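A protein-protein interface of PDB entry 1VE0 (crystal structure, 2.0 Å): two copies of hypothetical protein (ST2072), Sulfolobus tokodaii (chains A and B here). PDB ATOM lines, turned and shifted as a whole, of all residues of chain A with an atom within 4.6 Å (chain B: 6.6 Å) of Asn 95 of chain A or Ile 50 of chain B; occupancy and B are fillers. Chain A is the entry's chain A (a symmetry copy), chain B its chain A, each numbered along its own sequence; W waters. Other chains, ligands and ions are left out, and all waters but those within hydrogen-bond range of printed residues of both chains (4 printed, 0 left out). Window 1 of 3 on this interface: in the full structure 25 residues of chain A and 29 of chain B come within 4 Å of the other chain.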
ATOM      1  N   VAL A  39      24.824  -6.649  12.672  1.00  0.00           N
ATOM      2  CA  VAL A  39      23.483  -6.196  12.294  1.00  0.00           C
ATOM      3  C   VAL A  39      23.067  -5.285  13.438  1.00  0.00           C
ATOM      4  O   VAL A  39      22.839  -5.741  14.569  1.00  0.00           O
ATOM      5  CB  VAL A  39      22.522  -7.383  12.162  1.00  0.00           C
ATOM      6  CG1 VAL A  39      21.125  -6.906  11.757  1.00  0.00           C
ATOM      7  CG2 VAL A  39      23.073  -8.354  11.112  1.00  0.00           C
ATOM      8  N   ILE A  40      22.983  -3.998  13.123  1.00  0.00           N
ATOM      9  CA  ILE A  40      22.713  -2.963  14.117  1.00  0.00           C
ATOM     10  C   ILE A  40      21.535  -2.045  13.842  1.00  0.00           C
ATOM     11  O   ILE A  40      21.294  -1.673  12.700  1.00  0.00           O
ATOM     12  CB  ILE A  40      23.975  -2.045  14.229  1.00  0.00           C
ATOM     13  CG1 ILE A  40      25.181  -2.873  14.660  1.00  0.00           C
ATOM     14  CG2 ILE A  40      23.724  -0.859  15.181  1.00  0.00           C
ATOM     15  CD1 ILE A  40      26.489  -2.307  14.152  1.00  0.00           C
ATOM     16  N   VAL A  41      20.783  -1.685  14.877  1.00  0.00           N
ATOM     17  CA  VAL A  41      19.742  -0.683  14.662  1.00  0.00           C
ATOM     18  C   VAL A  41      20.178   0.483  15.531  1.00  0.00           C
ATOM     19  O   VAL A  41      20.672   0.284  16.643  1.00  0.00           O
ATOM     20  CB  VAL A  41      18.316  -1.129  15.075  1.00  0.00           C
ATOM     21  CG1 VAL A  41      17.789  -2.148  14.069  1.00  0.00           C
ATOM     22  CG2 VAL A  41      18.305  -1.673  16.522  1.00  0.00           C
ATOM     23  N   HIS A  43      18.241   2.425  16.757  1.00  0.00           N
ATOM     24  CA  HIS A  43      16.985   2.713  17.449  1.00  0.00           C
ATOM     25  C   HIS A  43      17.081   2.257  18.902  1.00  0.00           C
ATOM     26  O   HIS A  43      17.921   1.421  19.232  1.00  0.00           O
ATOM     27  CB  HIS A  43      15.842   1.964  16.773  1.00  0.00           C
ATOM     28  CG  HIS A  43      15.602   2.382  15.361  1.00  0.00           C
ATOM     29  ND1 HIS A  43      15.248   3.669  15.019  1.00  0.00           N
ATOM     30  CD2 HIS A  43      15.636   1.678  14.202  1.00  0.00           C
ATOM     31  CE1 HIS A  43      15.071   3.742  13.710  1.00  0.00           C
ATOM     32  NE2 HIS A  43      15.302   2.548  13.191  1.00  0.00           N
ATOM     33  N   ILE A  48      17.334  -6.618  17.829  1.00  0.00           N
ATOM     34  CA  ILE A  48      17.726  -7.632  16.847  1.00  0.00           C
ATOM     35  C   ILE A  48      18.064  -8.925  17.583  1.00  0.00           C
ATOM     36  O   ILE A  48      18.741  -8.899  18.609  1.00  0.00           O
ATOM     37  CB  ILE A  48      19.008  -7.202  16.039  1.00  0.00           C
ATOM     38  CG1 ILE A  48      18.732  -5.949  15.190  1.00  0.00           C
ATOM     39  CG2 ILE A  48      19.486  -8.348  15.146  1.00  0.00           C
ATOM     40  CD1 ILE A  48      17.700  -6.136  14.072  1.00  0.00           C
ATOM     41  N   SER A  90      14.102  -3.730  24.919  1.00  0.00           N
ATOM     42  CA  SER A  90      15.088  -3.573  23.842  1.00  0.00           C
ATOM     43  C   SER A  90      16.520  -3.452  24.385  1.00  0.00           C
ATOM     44  O   SER A  90      17.471  -3.917  23.754  1.00  0.00           O
ATOM     45  CB  SER A  90      14.784  -2.323  22.993  1.00  0.00           C
ATOM     46  OG  SER A  90      13.627  -2.499  22.177  1.00  0.00           O
ATOM     47  N   GLY A  94      19.197  -6.182  23.364  1.00  0.00           N
ATOM     48  CA  GLY A  94      20.321  -5.624  22.639  1.00  0.00           C
ATOM     49  C   GLY A  94      19.914  -5.073  21.284  1.00  0.00           C
ATOM     50  O   GLY A  94      18.956  -5.543  20.664  1.00  0.00           O
ATOM     51  N   ASN A  95      20.663  -4.090  20.800  1.00  0.00           N
ATOM     52  CA  ASN A  95      20.342  -3.470  19.519  1.00  0.00           C
ATOM     53  C   ASN A  95      21.175  -4.020  18.376  1.00  0.00           C
ATOM     54  O   ASN A  95      21.141  -3.479  17.274  1.00  0.00           O
ATOM     55  CB  ASN A  95      20.548  -1.964  19.603  1.00  0.00           C
ATOM     56  CG  ASN A  95      21.999  -1.601  19.784  1.00  0.00           C
ATOM     57  OD1 ASN A  95      22.665  -2.096  20.694  1.00  0.00           O
ATOM     58  ND2 ASN A  95      22.506  -0.736  18.908  1.00  0.00           N
ATOM     59  N   SER A  96      21.930  -5.083  18.636  1.00  0.00           N
ATOM     60  CA  SER A  96      22.739  -5.681  17.593  1.00  0.00           C
ATOM     61  C   SER A  96      22.983  -7.159  17.841  1.00  0.00           C
ATOM     62  O   SER A  96      22.800  -7.656  18.953  1.00  0.00           O
ATOM     63  CB  SER A  96      24.101  -4.978  17.479  1.00  0.00           C
ATOM     64  OG  SER A  96      24.908  -5.231  18.626  1.00  0.00           O
ATOM     65  N   VAL B  39      32.387  -2.041  23.321  1.00  0.00           N
ATOM     66  CA  VAL B  39      32.392  -1.467  24.669  1.00  0.00           C
ATOM     67  C   VAL B  39      32.203  -2.668  25.580  1.00  0.00           C
ATOM     68  O   VAL B  39      31.130  -3.290  25.607  1.00  0.00           O
ATOM     69  CB  VAL B  39      31.246  -0.463  24.840  1.00  0.00           C
ATOM     70  CG1 VAL B  39      31.263   0.142  26.245  1.00  0.00           C
ATOM     71  CG2 VAL B  39      31.392   0.642  23.788  1.00  0.00           C
ATOM     72  N   ILE B  48      26.411  -3.550  30.007  1.00  0.00           N
ATOM     73  CA  ILE B  48      26.423  -2.423  29.072  1.00  0.00           C
ATOM     74  C   ILE B  48      25.214  -2.537  28.148  1.00  0.00           C
ATOM     75  O   ILE B  48      24.903  -3.622  27.660  1.00  0.00           O
ATOM     76  CB  ILE B  48      27.710  -2.428  28.164  1.00  0.00           C
ATOM     77  CG1 ILE B  48      28.982  -2.226  29.006  1.00  0.00           C
ATOM     78  CG2 ILE B  48      27.611  -1.341  27.091  1.00  0.00           C
ATOM     79  CD1 ILE B  48      29.090  -0.865  29.703  1.00  0.00           C
ATOM     80  N   ILE B  49      24.516  -1.426  27.939  1.00  0.00           N
ATOM     81  CA  ILE B  49      23.370  -1.394  27.038  1.00  0.00           C
ATOM     82  C   ILE B  49      23.521  -0.119  26.232  1.00  0.00           C
ATOM     83  O   ILE B  49      24.259   0.777  26.649  1.00  0.00           O
ATOM     84  CB  ILE B  49      21.989  -1.280  27.767  1.00  0.00           C
ATOM     85  CG1 ILE B  49      21.892   0.061  28.514  1.00  0.00           C
ATOM     86  CG2 ILE B  49      21.780  -2.444  28.728  1.00  0.00           C
ATOM     87  CD1 ILE B  49      20.538   0.308  29.159  1.00  0.00           C
ATOM     88  N   ILE B  50      22.865  -0.062  25.073  1.00  0.00           N
ATOM     89  CA  ILE B  50      22.857   1.142  24.243  1.00  0.00           C
ATOM     90  C   ILE B  50      21.388   1.552  24.209  1.00  0.00           C
ATOM     91  O   ILE B  50      20.569   0.857  23.611  1.00  0.00           O
ATOM     92  CB  ILE B  50      23.291   0.895  22.775  1.00  0.00           C
ATOM     93  CG1 ILE B  50      24.645   0.195  22.715  1.00  0.00           C
ATOM     94  CG2 ILE B  50      23.363   2.240  22.017  1.00  0.00           C
ATOM     95  CD1 ILE B  50      25.756   0.924  23.441  1.00  0.00           C
ATOM     96  N   ASN B  51      21.044   2.660  24.861  1.00  0.00           N
ATOM     97  CA  ASN B  51      19.662   3.104  24.851  1.00  0.00           C
ATOM     98  C   ASN B  51      19.506   4.580  25.208  1.00  0.00           C
ATOM     99  O   ASN B  51      20.479   5.321  25.217  1.00  0.00           O
ATOM    100  CB  ASN B  51      18.827   2.218  25.779  1.00  0.00           C
ATOM    101  CG  ASN B  51      17.437   1.965  25.228  1.00  0.00           C
ATOM    102  OD1 ASN B  51      16.527   2.765  25.431  1.00  0.00           O
ATOM    103  ND2 ASN B  51      17.275   0.860  24.498  1.00  0.00           N
ATOM    104  N   GLU B  52      18.287   5.015  25.510  1.00  0.00           N
ATOM    105  CA  GLU B  52      18.088   6.431  25.812  1.00  0.00           C
ATOM    106  C   GLU B  52      18.367   6.743  27.276  1.00  0.00           C
ATOM    107  O   GLU B  52      17.881   6.058  28.177  1.00  0.00           O
ATOM    108  CB  GLU B  52      16.667   6.867  25.428  1.00  0.00           C
ATOM    109  CG  GLU B  52      16.437   8.371  25.564  1.00  0.00           C
ATOM    110  CD  GLU B  52      15.029   8.807  25.180  1.00  0.00           C
ATOM    111  OE1 GLU B  52      14.695   9.989  25.404  1.00  0.00           O
ATOM    112  OE2 GLU B  52      14.259   7.979  24.651  1.00  0.00           O
ATOM    113  N   ARG B  97      28.578  -4.299  24.170  1.00  0.00           N
ATOM    114  CA  ARG B  97      27.695  -3.783  23.132  1.00  0.00           C
ATOM    115  C   ARG B  97      28.617  -3.228  22.046  1.00  0.00           C
ATOM    116  O   ARG B  97      29.734  -2.799  22.343  1.00  0.00           O
ATOM    117  CB  ARG B  97      26.802  -2.654  23.674  1.00  0.00           C
ATOM    118  CG  ARG B  97      25.630  -3.135  24.521  1.00  0.00           C
ATOM    119  CD  ARG B  97      24.645  -3.915  23.662  1.00  0.00           C
ATOM    120  NE  ARG B  97      23.441  -4.285  24.403  1.00  0.00           N
ATOM    121  CZ  ARG B  97      23.357  -5.323  25.231  1.00  0.00           C
ATOM    122  NH1 ARG B  97      24.417  -6.104  25.439  1.00  0.00           N
ATOM    123  NH2 ARG B  97      22.198  -5.606  25.823  1.00  0.00           N
ATOM    124  N   VAL B  98      28.167  -3.252  20.797  1.00  0.00           N
ATOM    125  CA  VAL B  98      28.976  -2.712  19.718  1.00  0.00           C
ATOM    126  C   VAL B  98      28.399  -1.382  19.261  1.00  0.00           C
ATOM    127  O   VAL B  98      27.186  -1.175  19.288  1.00  0.00           O
ATOM    128  CB  VAL B  98      29.039  -3.667  18.509  1.00  0.00           C
ATOM    129  CG1 VAL B  98      29.697  -4.973  18.916  1.00  0.00           C
ATOM    130  CG2 VAL B  98      27.655  -3.934  17.990  1.00  0.00           C
ATOM    131  N   VAL B  99      29.278  -0.466  18.873  1.00  0.00           N
ATOM    132  CA  VAL B  99      28.841   0.830  18.379  1.00  0.00           C
ATOM    133  C   VAL B  99      29.675   1.073  17.133  1.00  0.00           C
ATOM    134  O   VAL B  99      30.894   0.938  17.152  1.00  0.00           O
ATOM    135  CB  VAL B  99      29.078   1.967  19.407  1.00  0.00           C
ATOM    136  CG1 VAL B  99      28.531   3.281  18.861  1.00  0.00           C
ATOM    137  CG2 VAL B  99      28.380   1.641  20.713  1.00  0.00           C
ATOM    138  N   PRO B 100      29.017   1.369  16.006  1.00  0.00           N
ATOM    139  CA  PRO B 100      29.824   1.603  14.808  1.00  0.00           C
ATOM    140  C   PRO B 100      30.511   2.957  14.908  1.00  0.00           C
ATOM    141  O   PRO B 100      30.039   3.847  15.609  1.00  0.00           O
ATOM    142  CB  PRO B 100      28.802   1.550  13.675  1.00  0.00           C
ATOM    143  CG  PRO B 100      27.525   2.049  14.350  1.00  0.00           C
ATOM    144  CD  PRO B 100      27.572   1.392  15.716  1.00  0.00           C
ATOM    145  N   LEU B 108      25.759   6.974  16.409  1.00  0.00           N
ATOM    146  CA  LEU B 108      24.604   6.755  17.274  1.00  0.00           C
ATOM    147  C   LEU B 108      23.308   7.355  16.745  1.00  0.00           C
ATOM    148  O   LEU B 108      23.316   8.404  16.099  1.00  0.00           O
ATOM    149  CB  LEU B 108      24.891   7.352  18.663  1.00  0.00           C
ATOM    150  CG  LEU B 108      26.079   6.717  19.395  1.00  0.00           C
ATOM    151  CD1 LEU B 108      26.604   7.625  20.517  1.00  0.00           C
ATOM    152  CD2 LEU B 108      25.636   5.375  19.926  1.00  0.00           C
ATOM    153  N   TRP B 111      18.377   9.019  19.805  1.00  0.00           N
ATOM    154  CA  TRP B 111      18.251   8.802  21.239  1.00  0.00           C
ATOM    155  C   TRP B 111      19.228   7.805  21.867  1.00  0.00           C
ATOM    156  O   TRP B 111      19.058   7.455  23.028  1.00  0.00           O
ATOM    157  CB  TRP B 111      16.818   8.356  21.560  1.00  0.00           C
ATOM    158  CG  TRP B 111      15.768   9.210  20.909  1.00  0.00           C
ATOM    159  CD1 TRP B 111      14.925   8.844  19.901  1.00  0.00           C
ATOM    160  CD2 TRP B 111      15.488  10.592  21.187  1.00  0.00           C
ATOM    161  NE1 TRP B 111      14.135   9.914  19.527  1.00  0.00           N
ATOM    162  CE2 TRP B 111      14.461  10.998  20.299  1.00  0.00           C
ATOM    163  CE3 TRP B 111      16.007  11.526  22.095  1.00  0.00           C
ATOM    164  CZ2 TRP B 111      13.943  12.300  20.294  1.00  0.00           C
ATOM    165  CZ3 TRP B 111      15.487  12.828  22.087  1.00  0.00           C
ATOM    166  CH2 TRP B 111      14.468  13.197  21.192  1.00  0.00           C
ATOM    167  N   GLN B 112      20.245   7.367  21.126  1.00  0.00           N
ATOM    168  CA  GLN B 112      21.194   6.392  21.668  1.00  0.00           C
ATOM    169  C   GLN B 112      22.357   6.934  22.473  1.00  0.00           C
ATOM    170  O   GLN B 112      23.078   7.843  22.045  1.00  0.00           O
ATOM    171  CB  GLN B 112      21.789   5.509  20.566  1.00  0.00           C
ATOM    172  CG  GLN B 112      20.856   4.514  19.942  1.00  0.00           C
ATOM    173  CD  GLN B 112      21.587   3.614  18.979  1.00  0.00           C
ATOM    174  OE1 GLN B 112      22.384   4.085  18.156  1.00  0.00           O
ATOM    175  NE2 GLN B 112      21.330   2.310  19.068  1.00  0.00           N
ATOM    176  N   ARG B 113      22.554   6.333  23.635  1.00  0.00           N
ATOM    177  CA  ARG B 113      23.654   6.680  24.515  1.00  0.00           C
ATOM    178  C   ARG B 113      24.213   5.337  24.996  1.00  0.00           C
ATOM    179  O   ARG B 113      23.515   4.330  25.003  1.00  0.00           O
ATOM    180  CB  ARG B 113      23.156   7.502  25.708  1.00  0.00           C
ATOM    181  CG  ARG B 113      22.459   8.826  25.312  1.00  0.00           C
ATOM    182  CD  ARG B 113      23.414   9.802  24.652  1.00  0.00           C
ATOM    183  NE  ARG B 113      24.374  10.355  25.602  1.00  0.00           N
ATOM    184  CZ  ARG B 113      25.283  11.281  25.299  1.00  0.00           C
ATOM    185  NH1 ARG B 113      26.116  11.722  26.233  1.00  0.00           N
ATOM    186  NH2 ARG B 113      25.365  11.771  24.063  1.00  0.00           N
ATOM    187  N   ILE B 114      25.479   5.323  25.366  1.00  0.00           N
ATOM    188  CA  ILE B 114      26.116   4.111  25.853  1.00  0.00           C
ATOM    189  C   ILE B 114      25.931   4.193  27.360  1.00  0.00           C
ATOM    190  O   ILE B 114      26.354   5.153  27.989  1.00  0.00           O
ATOM    191  CB  ILE B 114      27.594   4.101  25.467  1.00  0.00           C
ATOM    192  CG1 ILE B 114      27.700   4.193  23.935  1.00  0.00           C
ATOM    193  CG2 ILE B 114      28.268   2.812  25.990  1.00  0.00           C
ATOM    194  CD1 ILE B 114      29.114   4.317  23.410  1.00  0.00           C
ATOM    195  N   ILE B 115      25.280   3.191  27.932  1.00  0.00           N
ATOM    196  CA  ILE B 115      24.995   3.207  29.360  1.00  0.00           C
ATOM    197  C   ILE B 115      25.556   2.035  30.155  1.00  0.00           C
ATOM    198  O   ILE B 115      25.440   0.882  29.734  1.00  0.00           O
ATOM    199  CB  ILE B 115      23.460   3.237  29.569  1.00  0.00           C
ATOM    200  CG1 ILE B 115      22.883   4.508  28.934  1.00  0.00           C
ATOM    201  CG2 ILE B 115      23.125   3.142  31.051  1.00  0.00           C
ATOM    202  CD1 ILE B 115      21.399   4.442  28.666  1.00  0.00           C
HETATM  203  O   HOH W   1      18.958  -1.610  22.998  1.00  0.00           O
HETATM  204  O   HOH W   2      19.877   1.329  21.158  1.00  0.00           O
HETATM  205  O   HOH W   3      25.151   0.479  18.600  1.00  0.00           O
HETATM  206  O   HOH W   4      25.102  -3.029  20.056  1.00  0.00           O
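2 positions are printed for both chains. Of the 6 pairs that touch across the chains among the printed residues, none has its exchanged pair printed and touching as well.
Among the printed residues, merely in contact across the chains: Ser 96 of chain A with Val 98 of chain B (3.1 Å), His 43 of chain A with Gln 112 of chain B (3.5 Å), Asn 95 of chain A with Ile 50 of chain B (3.6 Å) and Gly 94 of chain A with Arg 97 of chain B (3.7 Å).
Of the printed residues of chain B, Val 41 of chain A touches Gln 112 (3.2 Å). Of the printed residues of chain B, His 43 of chain A touches Gln 112 (3.5 Å). Printed residues of chain B within 4 Å of Gly 94 of chain A: Arg 97 (3.7 Å). Printed residues of chain B within 4 Å of Asn 95 of chain A: Ile 50 (3.6 Å) and Gln 112 (3.3 Å). Ile 48 of chain B touches none of the printed residues of chain A. Printed residues of chain A within 4 Å of Val 98 of chain B: Ser 96. Trp 111 of chain B touches none of the printed residues of chain A. Printed residues of chain A within 4 Å of Gln 112 of chain B: Val 41, His 43 and Asn 95. The nearest printed residue of chain A that does not touch Ile 50 of chain B is His 43 of chain A (5.1 Å).
The side-chain amide nitrogen (NE2) of Gln 112 of chain B sits at hydrogen-bond distance from the backbone carbonyl oxygen (O) of Val 41 of chain A, at 3.2 Å. NE2 of Gln 112 of chain B lies close to ND2 of Asn 95 of chain A, 3.3 Å away.
Of the 9 printed residues of chain A, 5 touch a printed residue of chain B. Along chain A the printed residues that touch a printed residue of chain B span positions 41 to 96. Hydrophobic or aromatic side chains of chain B that line the printed part of chain A: Ile 50 and Val 98. Among the printed residues, 6 pairs touch across the chains. Among the printed residues, no Asp or Glu carboxylate lies within 4 Å of a Lys or Arg side-chain nitrogen of the other chain.
Water W2 lies within hydrogen-bond range of the backbone carbonyl oxygen of Ile 50 of chain B, the side-chain amide nitrogen of Gln 112 of chain B and the backbone carbonyl oxygen of His 43 of chain A. Water W4 lies within hydrogen-bond range of the side-chain hydroxyl (OG) of Ser 96 of chain A (2.6 Å), the side-chain amide oxygen (OD1) of Asn 95 of chain A (2.7 Å) and the backbone carbonyl oxygen (O) of Val 98 of chain B (2.9 Å). Water W3 lies within hydrogen-bond range of O of Val 98 of chain B and ND2 of Asn 95 of chain A. Water W1 lies within hydrogen-bond range of O of Ser 90 of chain A, O of Ile 50 of chain B and ND2 of Asn 51 of chain B.
The backbone carbonyl oxygen (O) of Arg 97 of chain B lies within hydrogen-bond range of the backbone NH (N) of Val 39 of chain B. The backbone carbonyl oxygen (O) of Gly 94 of chain A is in hydrogen-bond range of the backbone NH (N) of Ile 48 of chain A, 3.4 Å away. The backbone NH (N) of Val 41 of chain A sits at hydrogen-bond distance from the backbone carbonyl oxygen (O) of Asn 95 of chain A, at 3.0 Å. The backbone carbonyl oxygen (O) of Ile 48 of chain B sits close to the guanidinium group (NH1) of Arg 97 of chain B (3.4 Å).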
